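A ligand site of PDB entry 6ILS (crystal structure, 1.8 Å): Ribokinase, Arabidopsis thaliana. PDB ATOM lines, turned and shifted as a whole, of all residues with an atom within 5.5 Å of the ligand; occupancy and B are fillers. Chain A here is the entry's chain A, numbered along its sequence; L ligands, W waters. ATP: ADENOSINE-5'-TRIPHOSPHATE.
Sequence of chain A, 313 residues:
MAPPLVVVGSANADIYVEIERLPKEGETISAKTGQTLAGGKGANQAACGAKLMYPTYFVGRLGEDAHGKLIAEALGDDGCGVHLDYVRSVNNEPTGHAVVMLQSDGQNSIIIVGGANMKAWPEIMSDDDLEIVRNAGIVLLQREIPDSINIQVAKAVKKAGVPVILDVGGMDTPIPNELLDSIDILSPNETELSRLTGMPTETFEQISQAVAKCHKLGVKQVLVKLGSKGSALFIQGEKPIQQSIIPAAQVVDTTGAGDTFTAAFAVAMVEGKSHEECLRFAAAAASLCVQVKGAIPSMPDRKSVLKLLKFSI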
ATOM      1  N   LYS A  41       9.728 -34.883  24.553  1.00  0.00           N
ATOM      2  CA  LYS A  41       9.510 -33.857  23.541  1.00  0.00           C
ATOM      3  C   LYS A  41       8.244 -33.027  23.808  1.00  0.00           C
ATOM      4  O   LYS A  41       8.250 -31.805  23.632  1.00  0.00           O
ATOM      5  CB  LYS A  41       9.427 -34.478  22.153  1.00  0.00           C
ATOM      6  CG  LYS A  41      10.738 -35.110  21.700  1.00  0.00           C
ATOM      7  CD  LYS A  41      10.596 -35.668  20.287  1.00  0.00           C
ATOM      8  CE  LYS A  41      10.329 -34.565  19.284  1.00  0.00           C
ATOM      9  NZ  LYS A  41      11.539 -33.682  19.056  1.00  0.00           N
ATOM     10  N   ASP A 167       5.698 -32.977  14.826  1.00  0.00           N
ATOM     11  CA  ASP A 167       7.142 -33.245  14.938  1.00  0.00           C
ATOM     12  C   ASP A 167       7.392 -34.728  14.732  1.00  0.00           C
ATOM     13  O   ASP A 167       6.758 -35.578  15.358  1.00  0.00           O
ATOM     14  CB  ASP A 167       7.656 -32.787  16.318  1.00  0.00           C
ATOM     15  CG  ASP A 167       9.199 -32.782  16.430  1.00  0.00           C
ATOM     16  OD1 ASP A 167       9.895 -33.526  15.699  1.00  0.00           O
ATOM     17  OD2 ASP A 167       9.714 -32.020  17.277  1.00  0.00           O
ATOM     18  N   PRO A 188      10.155 -32.681  10.185  1.00  0.00           N
ATOM     19  CA  PRO A 188      11.236 -33.651  10.359  1.00  0.00           C
ATOM     20  C   PRO A 188      12.601 -32.962  10.350  1.00  0.00           C
ATOM     21  O   PRO A 188      12.718 -31.843   9.841  1.00  0.00           O
ATOM     22  CB  PRO A 188      11.066 -34.562   9.137  1.00  0.00           C
ATOM     23  CG  PRO A 188      10.597 -33.599   8.061  1.00  0.00           C
ATOM     24  CD  PRO A 188       9.829 -32.480   8.764  1.00  0.00           C
ATOM     25  N   ASN A 189      13.616 -33.600  10.917  1.00  0.00           N
ATOM     26  CA  ASN A 189      14.976 -33.156  10.617  1.00  0.00           C
ATOM     27  C   ASN A 189      15.408 -33.884   9.342  1.00  0.00           C
ATOM     28  O   ASN A 189      14.643 -34.671   8.784  1.00  0.00           O
ATOM     29  CB  ASN A 189      15.938 -33.412  11.791  1.00  0.00           C
ATOM     30  CG  ASN A 189      16.026 -34.873  12.197  1.00  0.00           C
ATOM     31  OD1 ASN A 189      15.754 -35.793  11.413  1.00  0.00           O
ATOM     32  ND2 ASN A 189      16.454 -35.110  13.442  1.00  0.00           N
ATOM     33  N   GLU A 190      16.635 -33.616   8.868  1.00  0.00           N
ATOM     34  CA  GLU A 190      17.111 -34.214   7.616  1.00  0.00           C
ATOM     35  C   GLU A 190      17.085 -35.736   7.631  1.00  0.00           C
ATOM     36  O   GLU A 190      16.700 -36.368   6.649  1.00  0.00           O
ATOM     37  CB  GLU A 190      18.532 -33.724   7.320  1.00  0.00           C
ATOM     38  CG  GLU A 190      19.434 -33.758   8.528  1.00  0.00           C
ATOM     39  CD  GLU A 190      20.345 -32.559   8.607  1.00  0.00           C
ATOM     40  OE1 GLU A 190      20.432 -31.807   7.604  1.00  0.00           O
ATOM     41  OE2 GLU A 190      20.946 -32.354   9.675  1.00  0.00           O
ATOM     42  N   GLU A 192      15.164 -37.713   9.553  1.00  0.00           N
ATOM     43  CA  GLU A 192      13.777 -38.151   9.632  1.00  0.00           C
ATOM     44  C   GLU A 192      13.058 -37.996   8.293  1.00  0.00           C
ATOM     45  O   GLU A 192      12.211 -38.811   7.945  1.00  0.00           O
ATOM     46  CB  GLU A 192      13.040 -37.365  10.718  1.00  0.00           C
ATOM     47  CG  GLU A 192      13.315 -37.882  12.119  1.00  0.00           C
ATOM     48  CD  GLU A 192      13.093 -36.837  13.186  1.00  0.00           C
ATOM     49  OE1 GLU A 192      12.679 -35.709  12.843  1.00  0.00           O
ATOM     50  OE2 GLU A 192      13.335 -37.151  14.364  1.00  0.00           O
ATOM     51  N   LYS A 225      14.012 -29.224   9.745  1.00  0.00           N
ATOM     52  CA  LYS A 225      15.061 -28.806  10.647  1.00  0.00           C
ATOM     53  C   LYS A 225      16.416 -29.310  10.124  1.00  0.00           C
ATOM     54  O   LYS A 225      16.581 -30.488   9.816  1.00  0.00           O
ATOM     55  CB  LYS A 225      14.763 -29.296  12.072  1.00  0.00           C
ATOM     56  CG  LYS A 225      13.543 -28.545  12.667  1.00  0.00           C
ATOM     57  CD  LYS A 225      13.070 -29.126  13.996  1.00  0.00           C
ATOM     58  CE  LYS A 225      12.373 -30.461  13.787  1.00  0.00           C
ATOM     59  NZ  LYS A 225      11.117 -30.576  14.594  1.00  0.00           N
ATOM     60  N   LEU A 226      17.366 -28.397  10.036  1.00  0.00           N
ATOM     61  CA  LEU A 226      18.611 -28.663   9.328  1.00  0.00           C
ATOM     62  C   LEU A 226      19.860 -28.578  10.198  1.00  0.00           C
ATOM     63  O   LEU A 226      20.979 -28.569   9.688  1.00  0.00           O
ATOM     64  CB  LEU A 226      18.746 -27.682   8.148  1.00  0.00           C
ATOM     65  CG  LEU A 226      17.633 -27.808   7.114  1.00  0.00           C
ATOM     66  CD1 LEU A 226      17.665 -26.659   6.108  1.00  0.00           C
ATOM     67  CD2 LEU A 226      17.740 -29.144   6.415  1.00  0.00           C
ATOM     68  N   GLY A 227      19.659 -28.536  11.512  1.00  0.00           N
ATOM     69  CA  GLY A 227      20.778 -28.441  12.442  1.00  0.00           C
ATOM     70  C   GLY A 227      21.596 -27.164  12.233  1.00  0.00           C
ATOM     71  O   GLY A 227      21.058 -26.062  12.297  1.00  0.00           O
ATOM     72  N   SER A 228      22.889 -27.326  11.980  1.00  0.00           N
ATOM     73  CA  SER A 228      23.776 -26.189  11.812  1.00  0.00           C
ATOM     74  C   SER A 228      23.435 -25.372  10.557  1.00  0.00           C
ATOM     75  O   SER A 228      23.813 -24.195  10.455  1.00  0.00           O
ATOM     76  CB  SER A 228      25.233 -26.640  11.752  1.00  0.00           C
ATOM     77  OG  SER A 228      25.478 -27.432  10.601  1.00  0.00           O
ATOM     78  N   GLY A 230      20.451 -24.504   9.735  1.00  0.00           N
ATOM     79  CA  GLY A 230      19.266 -23.705  10.006  1.00  0.00           C
ATOM     80  C   GLY A 230      17.982 -24.491   9.799  1.00  0.00           C
ATOM     81  O   GLY A 230      17.774 -25.528  10.412  1.00  0.00           O
ATOM     82  N   SER A 231      17.117 -23.981   8.921  1.00  0.00           N
ATOM     83  CA  SER A 231      15.832 -24.628   8.639  1.00  0.00           C
ATOM     84  C   SER A 231      15.272 -24.193   7.287  1.00  0.00           C
ATOM     85  O   SER A 231      15.757 -23.223   6.694  1.00  0.00           O
ATOM     86  CB  SER A 231      14.822 -24.292   9.733  1.00  0.00           C
ATOM     87  OG  SER A 231      14.682 -22.878   9.853  1.00  0.00           O
ATOM     88  N   ILE A 245      21.000 -20.529  10.946  1.00  0.00           N
ATOM     89  CA  ILE A 245      21.076 -20.375  12.379  1.00  0.00           C
ATOM     90  C   ILE A 245      21.430 -18.929  12.725  1.00  0.00           C
ATOM     91  O   ILE A 245      22.073 -18.234  11.939  1.00  0.00           O
ATOM     92  CB  ILE A 245      22.119 -21.324  12.983  1.00  0.00           C
ATOM     93  CG1 ILE A 245      23.528 -20.950  12.523  1.00  0.00           C
ATOM     94  CG2 ILE A 245      21.807 -22.747  12.602  1.00  0.00           C
ATOM     95  CD1 ILE A 245      24.605 -21.834  13.102  1.00  0.00           C
ATOM     96  N   ILE A 246      20.942 -18.464  13.866  1.00  0.00           N
ATOM     97  CA  ILE A 246      21.459 -17.265  14.479  1.00  0.00           C
ATOM     98  C   ILE A 246      22.576 -17.775  15.386  1.00  0.00           C
ATOM     99  O   ILE A 246      22.314 -18.322  16.457  1.00  0.00           O
ATOM    100  CB  ILE A 246      20.385 -16.472  15.257  1.00  0.00           C
ATOM    101  CG1 ILE A 246      19.314 -15.964  14.296  1.00  0.00           C
ATOM    102  CG2 ILE A 246      21.002 -15.321  16.011  1.00  0.00           C
ATOM    103  CD1 ILE A 246      18.243 -15.118  14.945  1.00  0.00           C
ATOM    104  N   PRO A 247      23.834 -17.630  14.925  1.00  0.00           N
ATOM    105  CA  PRO A 247      24.965 -18.334  15.548  1.00  0.00           C
ATOM    106  C   PRO A 247      25.083 -18.111  17.047  1.00  0.00           C
ATOM    107  O   PRO A 247      25.053 -16.974  17.543  1.00  0.00           O
ATOM    108  CB  PRO A 247      26.179 -17.753  14.814  1.00  0.00           C
ATOM    109  CG  PRO A 247      25.641 -17.362  13.473  1.00  0.00           C
ATOM    110  CD  PRO A 247      24.263 -16.829  13.765  1.00  0.00           C
ATOM    111  N   ALA A 248      25.175 -19.221  17.773  1.00  0.00           N
ATOM    112  CA  ALA A 248      25.419 -19.172  19.191  1.00  0.00           C
ATOM    113  C   ALA A 248      26.867 -18.797  19.422  1.00  0.00           C
ATOM    114  O   ALA A 248      27.747 -19.238  18.688  1.00  0.00           O
ATOM    115  CB  ALA A 248      25.113 -20.517  19.830  1.00  0.00           C
ATOM    116  N   VAL A 251      28.217 -23.265  21.724  1.00  0.00           N
ATOM    117  CA  VAL A 251      27.273 -24.374  21.815  1.00  0.00           C
ATOM    118  C   VAL A 251      27.605 -25.210  23.044  1.00  0.00           C
ATOM    119  O   VAL A 251      28.514 -26.031  23.020  1.00  0.00           O
ATOM    120  CB  VAL A 251      27.299 -25.254  20.558  1.00  0.00           C
ATOM    121  CG1 VAL A 251      26.282 -26.384  20.693  1.00  0.00           C
ATOM    122  CG2 VAL A 251      27.008 -24.415  19.332  1.00  0.00           C
ATOM    123  N   THR A 254      23.016 -29.011  22.881  1.00  0.00           N
ATOM    124  CA  THR A 254      21.912 -28.929  21.913  1.00  0.00           C
ATOM    125  C   THR A 254      20.645 -29.632  22.388  1.00  0.00           C
ATOM    126  O   THR A 254      19.661 -29.670  21.668  1.00  0.00           O
ATOM    127  CB  THR A 254      22.312 -29.520  20.559  1.00  0.00           C
ATOM    128  OG1 THR A 254      22.653 -30.896  20.733  1.00  0.00           O
ATOM    129  CG2 THR A 254      23.492 -28.771  19.964  1.00  0.00           C
ATOM    130  N   ALA A 257      16.870 -28.176  21.944  1.00  0.00           N
ATOM    131  CA  ALA A 257      16.842 -27.033  21.030  1.00  0.00           C
ATOM    132  C   ALA A 257      15.956 -27.246  19.809  1.00  0.00           C
ATOM    133  O   ALA A 257      15.369 -26.296  19.302  1.00  0.00           O
ATOM    134  CB  ALA A 257      18.263 -26.698  20.589  1.00  0.00           C
ATOM    135  N   GLY A 258      15.856 -28.479  19.329  1.00  0.00           N
ATOM    136  CA  GLY A 258      14.930 -28.761  18.248  1.00  0.00           C
ATOM    137  C   GLY A 258      13.497 -28.596  18.728  1.00  0.00           C
ATOM    138  O   GLY A 258      12.639 -28.080  18.020  1.00  0.00           O
ATOM    139  N   ASP A 259      13.236 -29.031  19.963  1.00  0.00           N
ATOM    140  CA  ASP A 259      11.933 -28.827  20.577  1.00  0.00           C
ATOM    141  C   ASP A 259      11.646 -27.342  20.743  1.00  0.00           C
ATOM    142  O   ASP A 259      10.519 -26.895  20.517  1.00  0.00           O
ATOM    143  CB  ASP A 259      11.859 -29.546  21.940  1.00  0.00           C
ATOM    144  CG  ASP A 259      11.892 -31.049  21.784  1.00  0.00           C
ATOM    145  OD1 ASP A 259      11.291 -31.552  20.811  1.00  0.00           O
ATOM    146  OD2 ASP A 259      12.526 -31.732  22.624  1.00  0.00           O
ATOM    147  N   PHE A 261      12.951 -24.901  18.923  1.00  0.00           N
ATOM    148  CA  PHE A 261      12.711 -24.378  17.569  1.00  0.00           C
ATOM    149  C   PHE A 261      11.262 -24.583  17.145  1.00  0.00           C
ATOM    150  O   PHE A 261      10.594 -23.646  16.718  1.00  0.00           O
ATOM    151  CB  PHE A 261      13.633 -25.044  16.545  1.00  0.00           C
ATOM    152  CG  PHE A 261      13.474 -24.490  15.151  1.00  0.00           C
ATOM    153  CD1 PHE A 261      12.549 -25.020  14.280  1.00  0.00           C
ATOM    154  CD2 PHE A 261      14.255 -23.421  14.728  1.00  0.00           C
ATOM    155  CE1 PHE A 261      12.388 -24.492  12.997  1.00  0.00           C
ATOM    156  CE2 PHE A 261      14.105 -22.888  13.458  1.00  0.00           C
ATOM    157  CZ  PHE A 261      13.173 -23.426  12.596  1.00  0.00           C
ATOM    158  N   ALA A 283      14.627 -19.611  15.138  1.00  0.00           N
ATOM    159  CA  ALA A 283      16.097 -19.623  15.116  1.00  0.00           C
ATOM    160  C   ALA A 283      16.700 -18.926  16.329  1.00  0.00           C
ATOM    161  O   ALA A 283      17.630 -19.439  16.951  1.00  0.00           O
ATOM    162  CB  ALA A 283      16.618 -18.968  13.816  1.00  0.00           C
ATOM    163  N   ALA A 286      16.063 -21.228  19.469  1.00  0.00           N
ATOM    164  CA  ALA A 286      16.952 -22.390  19.462  1.00  0.00           C
ATOM    165  C   ALA A 286      18.386 -22.001  19.785  1.00  0.00           C
ATOM    166  O   ALA A 286      19.118 -22.752  20.440  1.00  0.00           O
ATOM    167  CB  ALA A 286      16.902 -23.087  18.110  1.00  0.00           C
ATOM    168  N   SER A 287      18.783 -20.821  19.317  1.00  0.00           N
ATOM    169  CA  SER A 287      20.135 -20.317  19.532  1.00  0.00           C
ATOM    170  C   SER A 287      20.440 -20.065  20.998  1.00  0.00           C
ATOM    171  O   SER A 287      21.510 -20.410  21.487  1.00  0.00           O
ATOM    172  CB  SER A 287      20.344 -19.028  18.737  1.00  0.00           C
ATOM    173  OG  SER A 287      21.608 -18.457  19.044  1.00  0.00           O
ATOM    174  N   VAL A 290      20.803 -23.524  22.856  1.00  0.00           N
ATOM    175  CA  VAL A 290      22.014 -24.342  22.770  1.00  0.00           C
ATOM    176  C   VAL A 290      23.177 -23.759  23.571  1.00  0.00           C
ATOM    177  O   VAL A 290      24.210 -24.404  23.737  1.00  0.00           O
ATOM    178  CB  VAL A 290      22.494 -24.543  21.303  1.00  0.00           C
ATOM    179  CG1 VAL A 290      21.377 -25.136  20.429  1.00  0.00           C
ATOM    180  CG2 VAL A 290      23.013 -23.233  20.729  1.00  0.00           C
HETATM  181  PG  ATP L   1      15.832 -32.008  15.514  1.00  0.00           P
HETATM  182  O1G ATP L   1      16.822 -33.134  15.465  1.00  0.00           O
HETATM  183  O2G ATP L   1      15.663 -31.527  16.948  1.00  0.00           O
HETATM  184  O3G ATP L   1      14.511 -32.448  14.987  1.00  0.00           O
HETATM  185  PB  ATP L   1      17.877 -30.459  14.315  1.00  0.00           P
HETATM  186  O1B ATP L   1      18.415 -31.376  13.291  1.00  0.00           O
HETATM  187  O2B ATP L   1      17.972 -29.080  13.883  1.00  0.00           O
HETATM  188  O3B ATP L   1      16.357 -30.798  14.601  1.00  0.00           O
HETATM  189  PA  ATP L   1      19.944 -30.008  16.222  1.00  0.00           P
HETATM  190  O1A ATP L   1      20.245 -30.557  17.603  1.00  0.00           O
HETATM  191  O2A ATP L   1      21.095 -30.283  15.301  1.00  0.00           O
HETATM  192  O3A ATP L   1      18.661 -30.741  15.679  1.00  0.00           O
HETATM  193  O5' ATP L   1      19.650 -28.481  16.319  1.00  0.00           O
HETATM  194  C5' ATP L   1      18.661 -28.063  17.237  1.00  0.00           C
HETATM  195  C4' ATP L   1      18.156 -26.599  16.895  1.00  0.00           C
HETATM  196  O4' ATP L   1      19.216 -25.564  17.297  1.00  0.00           O
HETATM  197  C3' ATP L   1      17.941 -26.432  15.647  1.00  0.00           C
HETATM  198  O3' ATP L   1      16.868 -25.488  15.490  1.00  0.00           O
HETATM  199  C2' ATP L   1      19.310 -25.704  15.032  1.00  0.00           C
HETATM  200  O2' ATP L   1      18.938 -24.877  13.886  1.00  0.00           O
HETATM  201  C1' ATP L   1      19.784 -24.996  15.954  1.00  0.00           C
HETATM  202  N9  ATP L   1      21.249 -25.171  16.002  1.00  0.00           N
HETATM  203  C8  ATP L   1      22.176 -26.160  15.870  1.00  0.00           C
HETATM  204  N7  ATP L   1      23.397 -25.598  16.053  1.00  0.00           N
HETATM  205  C5  ATP L   1      23.228 -24.258  16.306  1.00  0.00           C
HETATM  206  C6  ATP L   1      24.148 -23.229  16.563  1.00  0.00           C
HETATM  207  N6  ATP L   1      25.572 -23.354  16.623  1.00  0.00           N
HETATM  208  N1  ATP L   1      23.720 -21.986  16.793  1.00  0.00           N
HETATM  209  C2  ATP L   1      22.358 -21.718  16.760  1.00  0.00           C
HETATM  210  N3  ATP L   1      21.462 -22.719  16.504  1.00  0.00           N
HETATM  211  C4  ATP L   1      21.897 -23.989  16.277  1.00  0.00           C
HETATM  212  O   HOH W   1      17.696 -30.753  19.503  1.00  0.00           O
HETATM  213  O   HOH W   2      16.342 -26.190  12.862  1.00  0.00           O
HETATM  214  O   HOH W   3      12.353 -33.627  14.818  1.00  0.00           O
HETATM  215  O   HOH W   4      19.539 -34.003  14.057  1.00  0.00           O
HETATM  216  O   HOH W   5      19.487 -20.850  15.384  1.00  0.00           O
HETATM  217  O   HOH W   6      17.951 -22.320  13.804  1.00  0.00           O
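Leu 226 touches the ligand. O of Gly 230 touches O2' of the ligand (3.7 Å). Ile 245 touches the ligand. O of Ile 246 touches C2 of the ligand (3.4 Å). CG2 of Val 251 touches N6 of the ligand (3.2 Å). Thr 254 touches the ligand. Ala 257 touches the ligand (CB to O4', 3.6 Å). Gly 258 touches the ligand. CD2 of Phe 261 touches O3' of the ligand (3.4 Å). Ala 286 touches the ligand (CB to O4', 3.5 Å). Ser 287 touches the ligand (CA to C2, 3.8 Å). CG1 of Val 290 touches O4' of the ligand (3.8 Å). Hydrophobic or aromatic side chains that line the ligand: Ile 245, Ala 248, Val 251, Ala 257, Phe 261, Ala 286 and Val 290. The nearest printed residue that does not touch the ligand is Pro 247 (4.1 Å).
The backbone carbonyl oxygen (O) of Lys 225 is in hydrogen-bond range of the backbone NH (N) of Glu 190, 3.3 Å away. The backbone NH of Glu 192 lies within hydrogen-bond range of the side-chain amide oxygen of Asn 189, 2.7 Å away. The backbone carbonyl oxygen (O) of Pro 188 sits at hydrogen-bond distance from the backbone NH (N) of Lys 225. O of Ile 246 sits at hydrogen-bond distance from OG of Ser 287 (2.7 Å). NZ of Lys 225 lies within salt-bridge range of OD2 of Asp 167 (3.4 Å).
An oxygen (O2B) of the ligand is in hydrogen-bond range of the backbone NH of Gly 227. The side-chain amino group (NZ) of Lys 225 is in salt-bridge range of an oxygen (O3G) of the ligand, at 3.9 Å. O1G of the ligand lies within hydrogen-bond range of ND2 of Asn 189, at 2.9 Å. The backbone NH (N) of Ala 248 sits at hydrogen-bond distance from a nitrogen (N1) of the ligand. O of Gly 227 is in hydrogen-bond range of O2' of the ligand, at 2.9 Å.
Water W3 lies within hydrogen-bond range of an oxygen (O3G) of the ligand, the side-chain carboxylate (OD1) of Asp 167, the side-chain carboxylate (OE1) of Glu 192 and the side-chain amino group (NZ) of Lys 225. Water W2 bridges an oxygen (O3') of the ligand (2.8 Å) and the backbone carbonyl oxygen of Gly 230 (2.9 Å). Water W5 lies within hydrogen-bond range of O of Ala 283 (2.8 Å), N3 of the ligand (2.9 Å) and N of Ile 246 (3.2 Å). Water W4 lies within hydrogen-bond range of O1B of the ligand (3.0 Å) and ND2 of Asn 189 (3.3 Å). Water W1 lies within hydrogen-bond range of the backbone NH of Gly 258 (2.9 Å), the backbone carbonyl oxygen of Thr 254 (3.1 Å) and an oxygen (O1A) of the ligand (3.2 Å).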
